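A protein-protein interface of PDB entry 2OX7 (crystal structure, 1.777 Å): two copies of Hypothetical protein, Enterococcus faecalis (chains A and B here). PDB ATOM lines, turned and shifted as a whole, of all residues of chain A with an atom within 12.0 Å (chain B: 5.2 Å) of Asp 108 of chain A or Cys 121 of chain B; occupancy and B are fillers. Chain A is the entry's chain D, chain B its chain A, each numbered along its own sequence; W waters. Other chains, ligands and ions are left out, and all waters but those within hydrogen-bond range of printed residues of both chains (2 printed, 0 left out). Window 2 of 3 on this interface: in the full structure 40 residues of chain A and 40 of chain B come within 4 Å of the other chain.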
ATOM      1  N   GLN A  69      17.557 -36.203  -6.912  1.00  0.00           N
ATOM      2  CA  GLN A  69      18.900 -35.752  -7.256  1.00  0.00           C
ATOM      3  C   GLN A  69      19.857 -35.926  -6.063  1.00  0.00           C
ATOM      4  O   GLN A  69      19.457 -35.800  -4.892  1.00  0.00           O
ATOM      5  CB  GLN A  69      18.894 -34.254  -7.642  1.00  0.00           C
ATOM      6  CG  GLN A  69      20.255 -33.813  -8.192  1.00  0.00           C
ATOM      7  CD  GLN A  69      20.241 -32.448  -8.859  1.00  0.00           C
ATOM      8  OE1 GLN A  69      19.181 -31.839  -9.068  1.00  0.00           O
ATOM      9  NE2 GLN A  69      21.426 -31.973  -9.209  1.00  0.00           N
ATOM     10  N   GLU A  83      18.091 -36.548  -2.313  1.00  0.00           N
ATOM     11  CA  GLU A  83      16.716 -36.183  -1.944  1.00  0.00           C
ATOM     12  C   GLU A  83      15.925 -37.440  -1.583  1.00  0.00           C
ATOM     13  O   GLU A  83      15.989 -38.477  -2.309  1.00  0.00           O
ATOM     14  CB  GLU A  83      16.016 -35.566  -3.140  1.00  0.00           C
ATOM     15  CG  GLU A  83      16.570 -34.263  -3.616  1.00  0.00           C
ATOM     16  CD  GLU A  83      15.699 -33.720  -4.735  1.00  0.00           C
ATOM     17  OE1 GLU A  83      15.778 -34.235  -5.873  1.00  0.00           O
ATOM     18  OE2 GLU A  83      14.881 -32.807  -4.428  1.00  0.00           O
ATOM     19  N   ILE A 104      15.833 -35.820   3.840  1.00  0.00           N
ATOM     20  CA  ILE A 104      16.530 -34.837   2.986  1.00  0.00           C
ATOM     21  C   ILE A 104      15.632 -34.292   1.882  1.00  0.00           C
ATOM     22  O   ILE A 104      14.979 -35.044   1.143  1.00  0.00           O
ATOM     23  CB  ILE A 104      17.713 -35.500   2.279  1.00  0.00           C
ATOM     24  CG1 ILE A 104      18.628 -36.149   3.329  1.00  0.00           C
ATOM     25  CG2 ILE A 104      18.423 -34.506   1.372  1.00  0.00           C
ATOM     26  CD1 ILE A 104      19.169 -35.218   4.402  1.00  0.00           C
ATOM     27  N   ALA A 105      15.611 -32.960   1.763  1.00  0.00           N
ATOM     28  CA  ALA A 105      14.823 -32.323   0.724  1.00  0.00           C
ATOM     29  C   ALA A 105      15.600 -31.159   0.137  1.00  0.00           C
ATOM     30  O   ALA A 105      16.652 -30.811   0.675  1.00  0.00           O
ATOM     31  CB  ALA A 105      13.486 -31.860   1.304  1.00  0.00           C
ATOM     32  N   TYR A 106      15.103 -30.616  -0.981  1.00  0.00           N
ATOM     33  CA  TYR A 106      15.654 -29.362  -1.527  1.00  0.00           C
ATOM     34  C   TYR A 106      14.533 -28.329  -1.472  1.00  0.00           C
ATOM     35  O   TYR A 106      13.368 -28.644  -1.743  1.00  0.00           O
ATOM     36  CB  TYR A 106      16.099 -29.533  -2.961  1.00  0.00           C
ATOM     37  CG  TYR A 106      16.620 -28.245  -3.573  1.00  0.00           C
ATOM     38  CD1 TYR A 106      17.978 -27.947  -3.521  1.00  0.00           C
ATOM     39  CD2 TYR A 106      15.755 -27.335  -4.197  1.00  0.00           C
ATOM     40  CE1 TYR A 106      18.490 -26.759  -4.063  1.00  0.00           C
ATOM     41  CE2 TYR A 106      16.243 -26.127  -4.727  1.00  0.00           C
ATOM     42  CZ  TYR A 106      17.604 -25.859  -4.650  1.00  0.00           C
ATOM     43  OH  TYR A 106      18.088 -24.716  -5.183  1.00  0.00           O
ATOM     44  N   ALA A 107      14.863 -27.103  -1.091  1.00  0.00           N
ATOM     45  CA  ALA A 107      13.879 -26.018  -1.277  1.00  0.00           C
ATOM     46  C   ALA A 107      14.609 -24.721  -1.129  1.00  0.00           C
ATOM     47  O   ALA A 107      15.524 -24.603  -0.304  1.00  0.00           O
ATOM     48  CB  ALA A 107      12.809 -26.083  -0.256  1.00  0.00           C
ATOM     49  N   ASP A 108      14.200 -23.781  -1.966  1.00  0.00           N
ATOM     50  CA  ASP A 108      14.578 -22.397  -1.774  1.00  0.00           C
ATOM     51  C   ASP A 108      16.093 -22.184  -1.723  1.00  0.00           C
ATOM     52  O   ASP A 108      16.577 -21.356  -0.926  1.00  0.00           O
ATOM     53  CB  ASP A 108      13.880 -21.860  -0.510  1.00  0.00           C
ATOM     54  CG  ASP A 108      13.709 -20.345  -0.543  1.00  0.00           C
ATOM     55  OD1 ASP A 108      13.612 -19.765  -1.662  1.00  0.00           O
ATOM     56  OD2 ASP A 108      13.621 -19.768   0.545  1.00  0.00           O
ATOM     57  N   GLY A 109      16.825 -22.903  -2.587  1.00  0.00           N
ATOM     58  CA  GLY A 109      18.249 -22.681  -2.741  1.00  0.00           C
ATOM     59  C   GLY A 109      19.191 -23.660  -2.058  1.00  0.00           C
ATOM     60  O   GLY A 109      20.405 -23.556  -2.240  1.00  0.00           O
ATOM     61  N   ARG A 110      18.649 -24.572  -1.242  1.00  0.00           N
ATOM     62  CA  ARG A 110      19.518 -25.489  -0.492  1.00  0.00           C
ATOM     63  C   ARG A 110      18.872 -26.850  -0.335  1.00  0.00           C
ATOM     64  O   ARG A 110      17.636 -26.970  -0.345  1.00  0.00           O
ATOM     65  CB  ARG A 110      19.890 -24.949   0.913  1.00  0.00           C
ATOM     66  CG  ARG A 110      18.635 -24.730   1.805  1.00  0.00           C
ATOM     67  CD  ARG A 110      18.898 -24.533   3.287  1.00  0.00           C
ATOM     68  NE  ARG A 110      17.613 -24.605   3.977  1.00  0.00           N
ATOM     69  CZ  ARG A 110      17.438 -24.788   5.284  1.00  0.00           C
ATOM     70  NH1 ARG A 110      18.476 -24.912   6.119  1.00  0.00           N
ATOM     71  NH2 ARG A 110      16.207 -24.842   5.748  1.00  0.00           N
ATOM     72  N   PHE A 111      19.744 -27.858  -0.259  1.00  0.00           N
ATOM     73  CA  PHE A 111      19.381 -29.140   0.320  1.00  0.00           C
ATOM     74  C   PHE A 111      19.422 -28.995   1.829  1.00  0.00           C
ATOM     75  O   PHE A 111      20.259 -28.250   2.392  1.00  0.00           O
ATOM     76  CB  PHE A 111      20.343 -30.255  -0.114  1.00  0.00           C
ATOM     77  CG  PHE A 111      20.328 -30.555  -1.575  1.00  0.00           C
ATOM     78  CD1 PHE A 111      19.312 -31.364  -2.123  1.00  0.00           C
ATOM     79  CD2 PHE A 111      21.340 -30.080  -2.402  1.00  0.00           C
ATOM     80  CE1 PHE A 111      19.300 -31.662  -3.482  1.00  0.00           C
ATOM     81  CE2 PHE A 111      21.351 -30.371  -3.771  1.00  0.00           C
ATOM     82  CZ  PHE A 111      20.323 -31.188  -4.302  1.00  0.00           C
ATOM     83  N   PHE A 112      18.497 -29.666   2.500  1.00  0.00           N
ATOM     84  CA  PHE A 112      18.456 -29.641   3.960  1.00  0.00           C
ATOM     85  C   PHE A 112      17.894 -30.916   4.530  1.00  0.00           C
ATOM     86  O   PHE A 112      17.305 -31.709   3.812  1.00  0.00           O
ATOM     87  CB  PHE A 112      17.669 -28.460   4.462  1.00  0.00           C
ATOM     88  CG  PHE A 112      16.254 -28.470   3.995  1.00  0.00           C
ATOM     89  CD1 PHE A 112      15.257 -28.850   4.857  1.00  0.00           C
ATOM     90  CD2 PHE A 112      15.934 -28.108   2.678  1.00  0.00           C
ATOM     91  CE1 PHE A 112      13.898 -28.879   4.410  1.00  0.00           C
ATOM     92  CE2 PHE A 112      14.597 -28.124   2.242  1.00  0.00           C
ATOM     93  CZ  PHE A 112      13.602 -28.511   3.098  1.00  0.00           C
ATOM     94  N   TRP A 113      18.141 -31.114   5.817  1.00  0.00           N
ATOM     95  CA  TRP A 113      17.557 -32.231   6.559  1.00  0.00           C
ATOM     96  C   TRP A 113      16.455 -31.660   7.452  1.00  0.00           C
ATOM     97  O   TRP A 113      16.601 -30.590   8.077  1.00  0.00           O
ATOM     98  CB  TRP A 113      18.579 -33.004   7.387  1.00  0.00           C
ATOM     99  CG  TRP A 113      19.681 -32.265   8.068  1.00  0.00           C
ATOM    100  CD1 TRP A 113      19.701 -30.964   8.482  1.00  0.00           C
ATOM    101  CD2 TRP A 113      20.949 -32.831   8.431  1.00  0.00           C
ATOM    102  NE1 TRP A 113      20.928 -30.675   9.068  1.00  0.00           N
ATOM    103  CE2 TRP A 113      21.699 -31.816   9.061  1.00  0.00           C
ATOM    104  CE3 TRP A 113      21.512 -34.118   8.286  1.00  0.00           C
ATOM    105  CZ2 TRP A 113      23.010 -32.028   9.537  1.00  0.00           C
ATOM    106  CZ3 TRP A 113      22.827 -34.338   8.746  1.00  0.00           C
ATOM    107  CH2 TRP A 113      23.552 -33.295   9.375  1.00  0.00           C
ATOM    108  N   GLU A 114      15.342 -32.364   7.485  1.00  0.00           N
ATOM    109  CA  GLU A 114      14.209 -31.898   8.253  1.00  0.00           C
ATOM    110  C   GLU A 114      14.332 -32.136   9.739  1.00  0.00           C
ATOM    111  O   GLU A 114      14.969 -33.101  10.182  1.00  0.00           O
ATOM    112  CB  GLU A 114      12.954 -32.485   7.647  1.00  0.00           C
ATOM    113  CG  GLU A 114      12.794 -32.043   6.211  1.00  0.00           C
ATOM    114  CD  GLU A 114      11.546 -32.597   5.571  1.00  0.00           C
ATOM    115  OE1 GLU A 114      10.712 -33.122   6.331  1.00  0.00           O
ATOM    116  OE2 GLU A 114      11.395 -32.506   4.326  1.00  0.00           O
ATOM    117  N   PHE A 120      22.918 -28.311   7.072  1.00  0.00           N
ATOM    118  CA  PHE A 120      23.229 -29.549   6.326  1.00  0.00           C
ATOM    119  C   PHE A 120      24.440 -29.264   5.476  1.00  0.00           C
ATOM    120  O   PHE A 120      24.372 -28.494   4.477  1.00  0.00           O
ATOM    121  CB  PHE A 120      22.003 -29.937   5.480  1.00  0.00           C
ATOM    122  CG  PHE A 120      22.222 -31.138   4.591  1.00  0.00           C
ATOM    123  CD1 PHE A 120      22.285 -32.405   5.116  1.00  0.00           C
ATOM    124  CD2 PHE A 120      22.324 -30.968   3.216  1.00  0.00           C
ATOM    125  CE1 PHE A 120      22.481 -33.524   4.262  1.00  0.00           C
ATOM    126  CE2 PHE A 120      22.502 -32.071   2.366  1.00  0.00           C
ATOM    127  CZ  PHE A 120      22.596 -33.344   2.911  1.00  0.00           C
ATOM    128  N   LEU B  73      15.368 -20.667  -8.489  1.00  0.00           N
ATOM    129  CA  LEU B  73      14.930 -19.358  -7.998  1.00  0.00           C
ATOM    130  C   LEU B  73      14.872 -18.375  -9.148  1.00  0.00           C
ATOM    131  O   LEU B  73      15.602 -18.536 -10.137  1.00  0.00           O
ATOM    132  CB  LEU B  73      15.882 -18.848  -6.929  1.00  0.00           C
ATOM    133  CG  LEU B  73      16.009 -19.803  -5.710  1.00  0.00           C
ATOM    134  CD1 LEU B  73      17.137 -19.317  -4.830  1.00  0.00           C
ATOM    135  CD2 LEU B  73      14.686 -19.979  -4.963  1.00  0.00           C
ATOM    136  N   TRP B 113      25.176 -16.742  -3.317  1.00  0.00           N
ATOM    137  CA  TRP B 113      25.803 -15.617  -4.013  1.00  0.00           C
ATOM    138  C   TRP B 113      27.097 -15.277  -3.310  1.00  0.00           C
ATOM    139  O   TRP B 113      27.163 -15.101  -2.085  1.00  0.00           O
ATOM    140  CB  TRP B 113      24.882 -14.403  -4.093  1.00  0.00           C
ATOM    141  CG  TRP B 113      23.977 -14.171  -2.945  1.00  0.00           C
ATOM    142  CD1 TRP B 113      24.197 -14.452  -1.637  1.00  0.00           C
ATOM    143  CD2 TRP B 113      22.695 -13.519  -3.023  1.00  0.00           C
ATOM    144  NE1 TRP B 113      23.103 -14.057  -0.876  1.00  0.00           N
ATOM    145  CE2 TRP B 113      22.152 -13.506  -1.708  1.00  0.00           C
ATOM    146  CE3 TRP B 113      21.922 -13.022  -4.099  1.00  0.00           C
ATOM    147  CZ2 TRP B 113      20.882 -12.929  -1.403  1.00  0.00           C
ATOM    148  CZ3 TRP B 113      20.629 -12.458  -3.804  1.00  0.00           C
ATOM    149  CH2 TRP B 113      20.129 -12.425  -2.460  1.00  0.00           C
ATOM    150  N   VAL B 119      21.263 -14.681   3.265  1.00  0.00           N
ATOM    151  CA  VAL B 119      20.797 -16.001   2.916  1.00  0.00           C
ATOM    152  C   VAL B 119      20.336 -15.907   1.457  1.00  0.00           C
ATOM    153  O   VAL B 119      19.531 -15.052   1.087  1.00  0.00           O
ATOM    154  CB  VAL B 119      19.616 -16.399   3.841  1.00  0.00           C
ATOM    155  CG1 VAL B 119      18.972 -17.705   3.400  1.00  0.00           C
ATOM    156  CG2 VAL B 119      20.093 -16.497   5.357  1.00  0.00           C
ATOM    157  N   PHE B 120      20.869 -16.761   0.617  1.00  0.00           N
ATOM    158  CA  PHE B 120      20.386 -16.812  -0.777  1.00  0.00           C
ATOM    159  C   PHE B 120      19.102 -17.615  -0.784  1.00  0.00           C
ATOM    160  O   PHE B 120      19.108 -18.872  -0.689  1.00  0.00           O
ATOM    161  CB  PHE B 120      21.459 -17.472  -1.651  1.00  0.00           C
ATOM    162  CG  PHE B 120      21.097 -17.557  -3.111  1.00  0.00           C
ATOM    163  CD1 PHE B 120      20.943 -16.405  -3.860  1.00  0.00           C
ATOM    164  CD2 PHE B 120      20.940 -18.804  -3.722  1.00  0.00           C
ATOM    165  CE1 PHE B 120      20.620 -16.455  -5.217  1.00  0.00           C
ATOM    166  CE2 PHE B 120      20.625 -18.868  -5.104  1.00  0.00           C
ATOM    167  CZ  PHE B 120      20.473 -17.692  -5.830  1.00  0.00           C
ATOM    168  N   CYS B 121      17.975 -16.905  -0.913  1.00  0.00           N
ATOM    169  CA  CYS B 121      16.672 -17.531  -0.940  1.00  0.00           C
ATOM    170  C   CYS B 121      15.726 -16.602  -1.742  1.00  0.00           C
ATOM    171  O   CYS B 121      16.072 -15.434  -2.010  1.00  0.00           O
ATOM    172  CB  CYS B 121      16.133 -17.754   0.504  1.00  0.00           C
ATOM    173  SG  CYS B 121      15.936 -16.240   1.418  1.00  0.00           S
ATOM    174  N   GLN B 122      14.572 -17.123  -2.122  1.00  0.00           N
ATOM    175  CA  GLN B 122      13.703 -16.364  -3.031  1.00  0.00           C
ATOM    176  C   GLN B 122      13.294 -15.013  -2.433  1.00  0.00           C
ATOM    177  O   GLN B 122      13.238 -14.002  -3.129  1.00  0.00           O
ATOM    178  CB  GLN B 122      12.477 -17.170  -3.392  1.00  0.00           C
ATOM    179  CG  GLN B 122      11.600 -16.449  -4.446  1.00  0.00           C
ATOM    180  CD  GLN B 122      12.342 -16.348  -5.787  1.00  0.00           C
ATOM    181  OE1 GLN B 122      12.322 -17.298  -6.585  1.00  0.00           O
ATOM    182  NE2 GLN B 122      12.999 -15.232  -6.029  1.00  0.00           N
ATOM    183  N   SER B 123      12.966 -14.993  -1.153  1.00  0.00           N
ATOM    184  CA  SER B 123      12.448 -13.744  -0.577  1.00  0.00           C
ATOM    185  C   SER B 123      13.575 -12.695  -0.482  1.00  0.00           C
ATOM    186  O   SER B 123      13.310 -11.489  -0.691  1.00  0.00           O
ATOM    187  CB  SER B 123      11.808 -14.026   0.812  1.00  0.00           C
ATOM    188  OG  SER B 123      12.821 -14.358   1.729  1.00  0.00           O
ATOM    189  N   ASN B 124      14.821 -13.114  -0.202  1.00  0.00           N
ATOM    190  CA  ASN B 124      15.929 -12.146  -0.205  1.00  0.00           C
ATOM    191  C   ASN B 124      16.269 -11.609  -1.598  1.00  0.00           C
ATOM    192  O   ASN B 124      16.671 -10.425  -1.774  1.00  0.00           O
ATOM    193  CB  ASN B 124      17.211 -12.700   0.394  1.00  0.00           C
ATOM    194  CG  ASN B 124      17.403 -12.256   1.842  1.00  0.00           C
ATOM    195  OD1 ASN B 124      16.952 -11.171   2.256  1.00  0.00           O
ATOM    196  ND2 ASN B 124      18.130 -13.081   2.598  1.00  0.00           N
ATOM    197  N   ILE B 125      16.085 -12.462  -2.586  1.00  0.00           N
ATOM    198  CA  ILE B 125      16.307 -12.013  -3.981  1.00  0.00           C
ATOM    199  C   ILE B 125      15.338 -10.871  -4.344  1.00  0.00           C
ATOM    200  O   ILE B 125      15.678  -9.959  -5.097  1.00  0.00           O
ATOM    201  CB  ILE B 125      16.226 -13.204  -4.969  1.00  0.00           C
ATOM    202  CG1 ILE B 125      17.396 -14.196  -4.749  1.00  0.00           C
ATOM    203  CG2 ILE B 125      16.251 -12.712  -6.434  1.00  0.00           C
ATOM    204  CD1 ILE B 125      17.083 -15.579  -5.307  1.00  0.00           C
HETATM  205  O   HOH W   1      12.250 -17.490   0.373  1.00  0.00           O
HETATM  206  O   HOH W   2      20.856 -20.959  -0.264  1.00  0.00           O
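OD1 of Asp 108 of chain A sits at hydrogen-bond distance from N of Gln 122 of chain B (2.8 Å).
The side-chain hydroxyl (OG) of Ser 123 of chain B is in hydrogen-bond range of the side-chain sulfur (SG) of Cys 121 of chain B (3.7 Å).
N of Asn 124 of chain B sits at hydrogen-bond distance from SG of Cys 121 of chain B (3.7 Å).
Among the printed residues, merely in contact across the chains: Asp 108 of chain A with Leu 73 of chain B (3.5 Å), Asp 108 of chain A with Phe 120 of chain B (3.6 Å) and Asp 108 of chain A with Cys 121 of chain B (3.2 Å).
Of chain B, only Leu 73 (3.5 Å), Phe 120 (3.6 Å), Cys 121 (3.2 Å) and Gln 122 (2.8 Å) come within 4 Å of Asp 108 of chain A.
Cys 121 of chain B touches just one residue of chain A: Asp 108.
No residue of chain A comes within 4 Å of Val 119 of chain B.
Of chain A, only Asp 108 comes within 4 Å of Phe 120 of chain B.
No residue of chain A comes within 4 Å of Asn 124 of chain B.
Printed residues of chain A within 4 Å of Leu 73 of chain B: Asp 108.
The nearest printed residue of chain A that does not touch Leu 73 of chain B is Gly 109 of chain A (4.1 Å).
Hydrophobic or aromatic side chains of chain B that line the printed part of chain A: Leu 73.
Of the 14 printed residues of chain A, 1 touches a printed residue of chain B.
Among the printed residues, no Asp or Glu carboxylate lies within 4 Å of a Lys or Arg side-chain nitrogen of the other chain.
2 positions are printed for both chains.
Water W1 lies within hydrogen-bond range of OD2 of Asp 108 of chain A (2.7 Å), N of Ser 123 of chain B (3.0 Å) and N of Gln 122 of chain B (3.4 Å).
Water W2 lies within hydrogen-bond range of O of Phe 120 of chain B (2.8 Å) and O of Gly 109 of chain A (3.3 Å).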
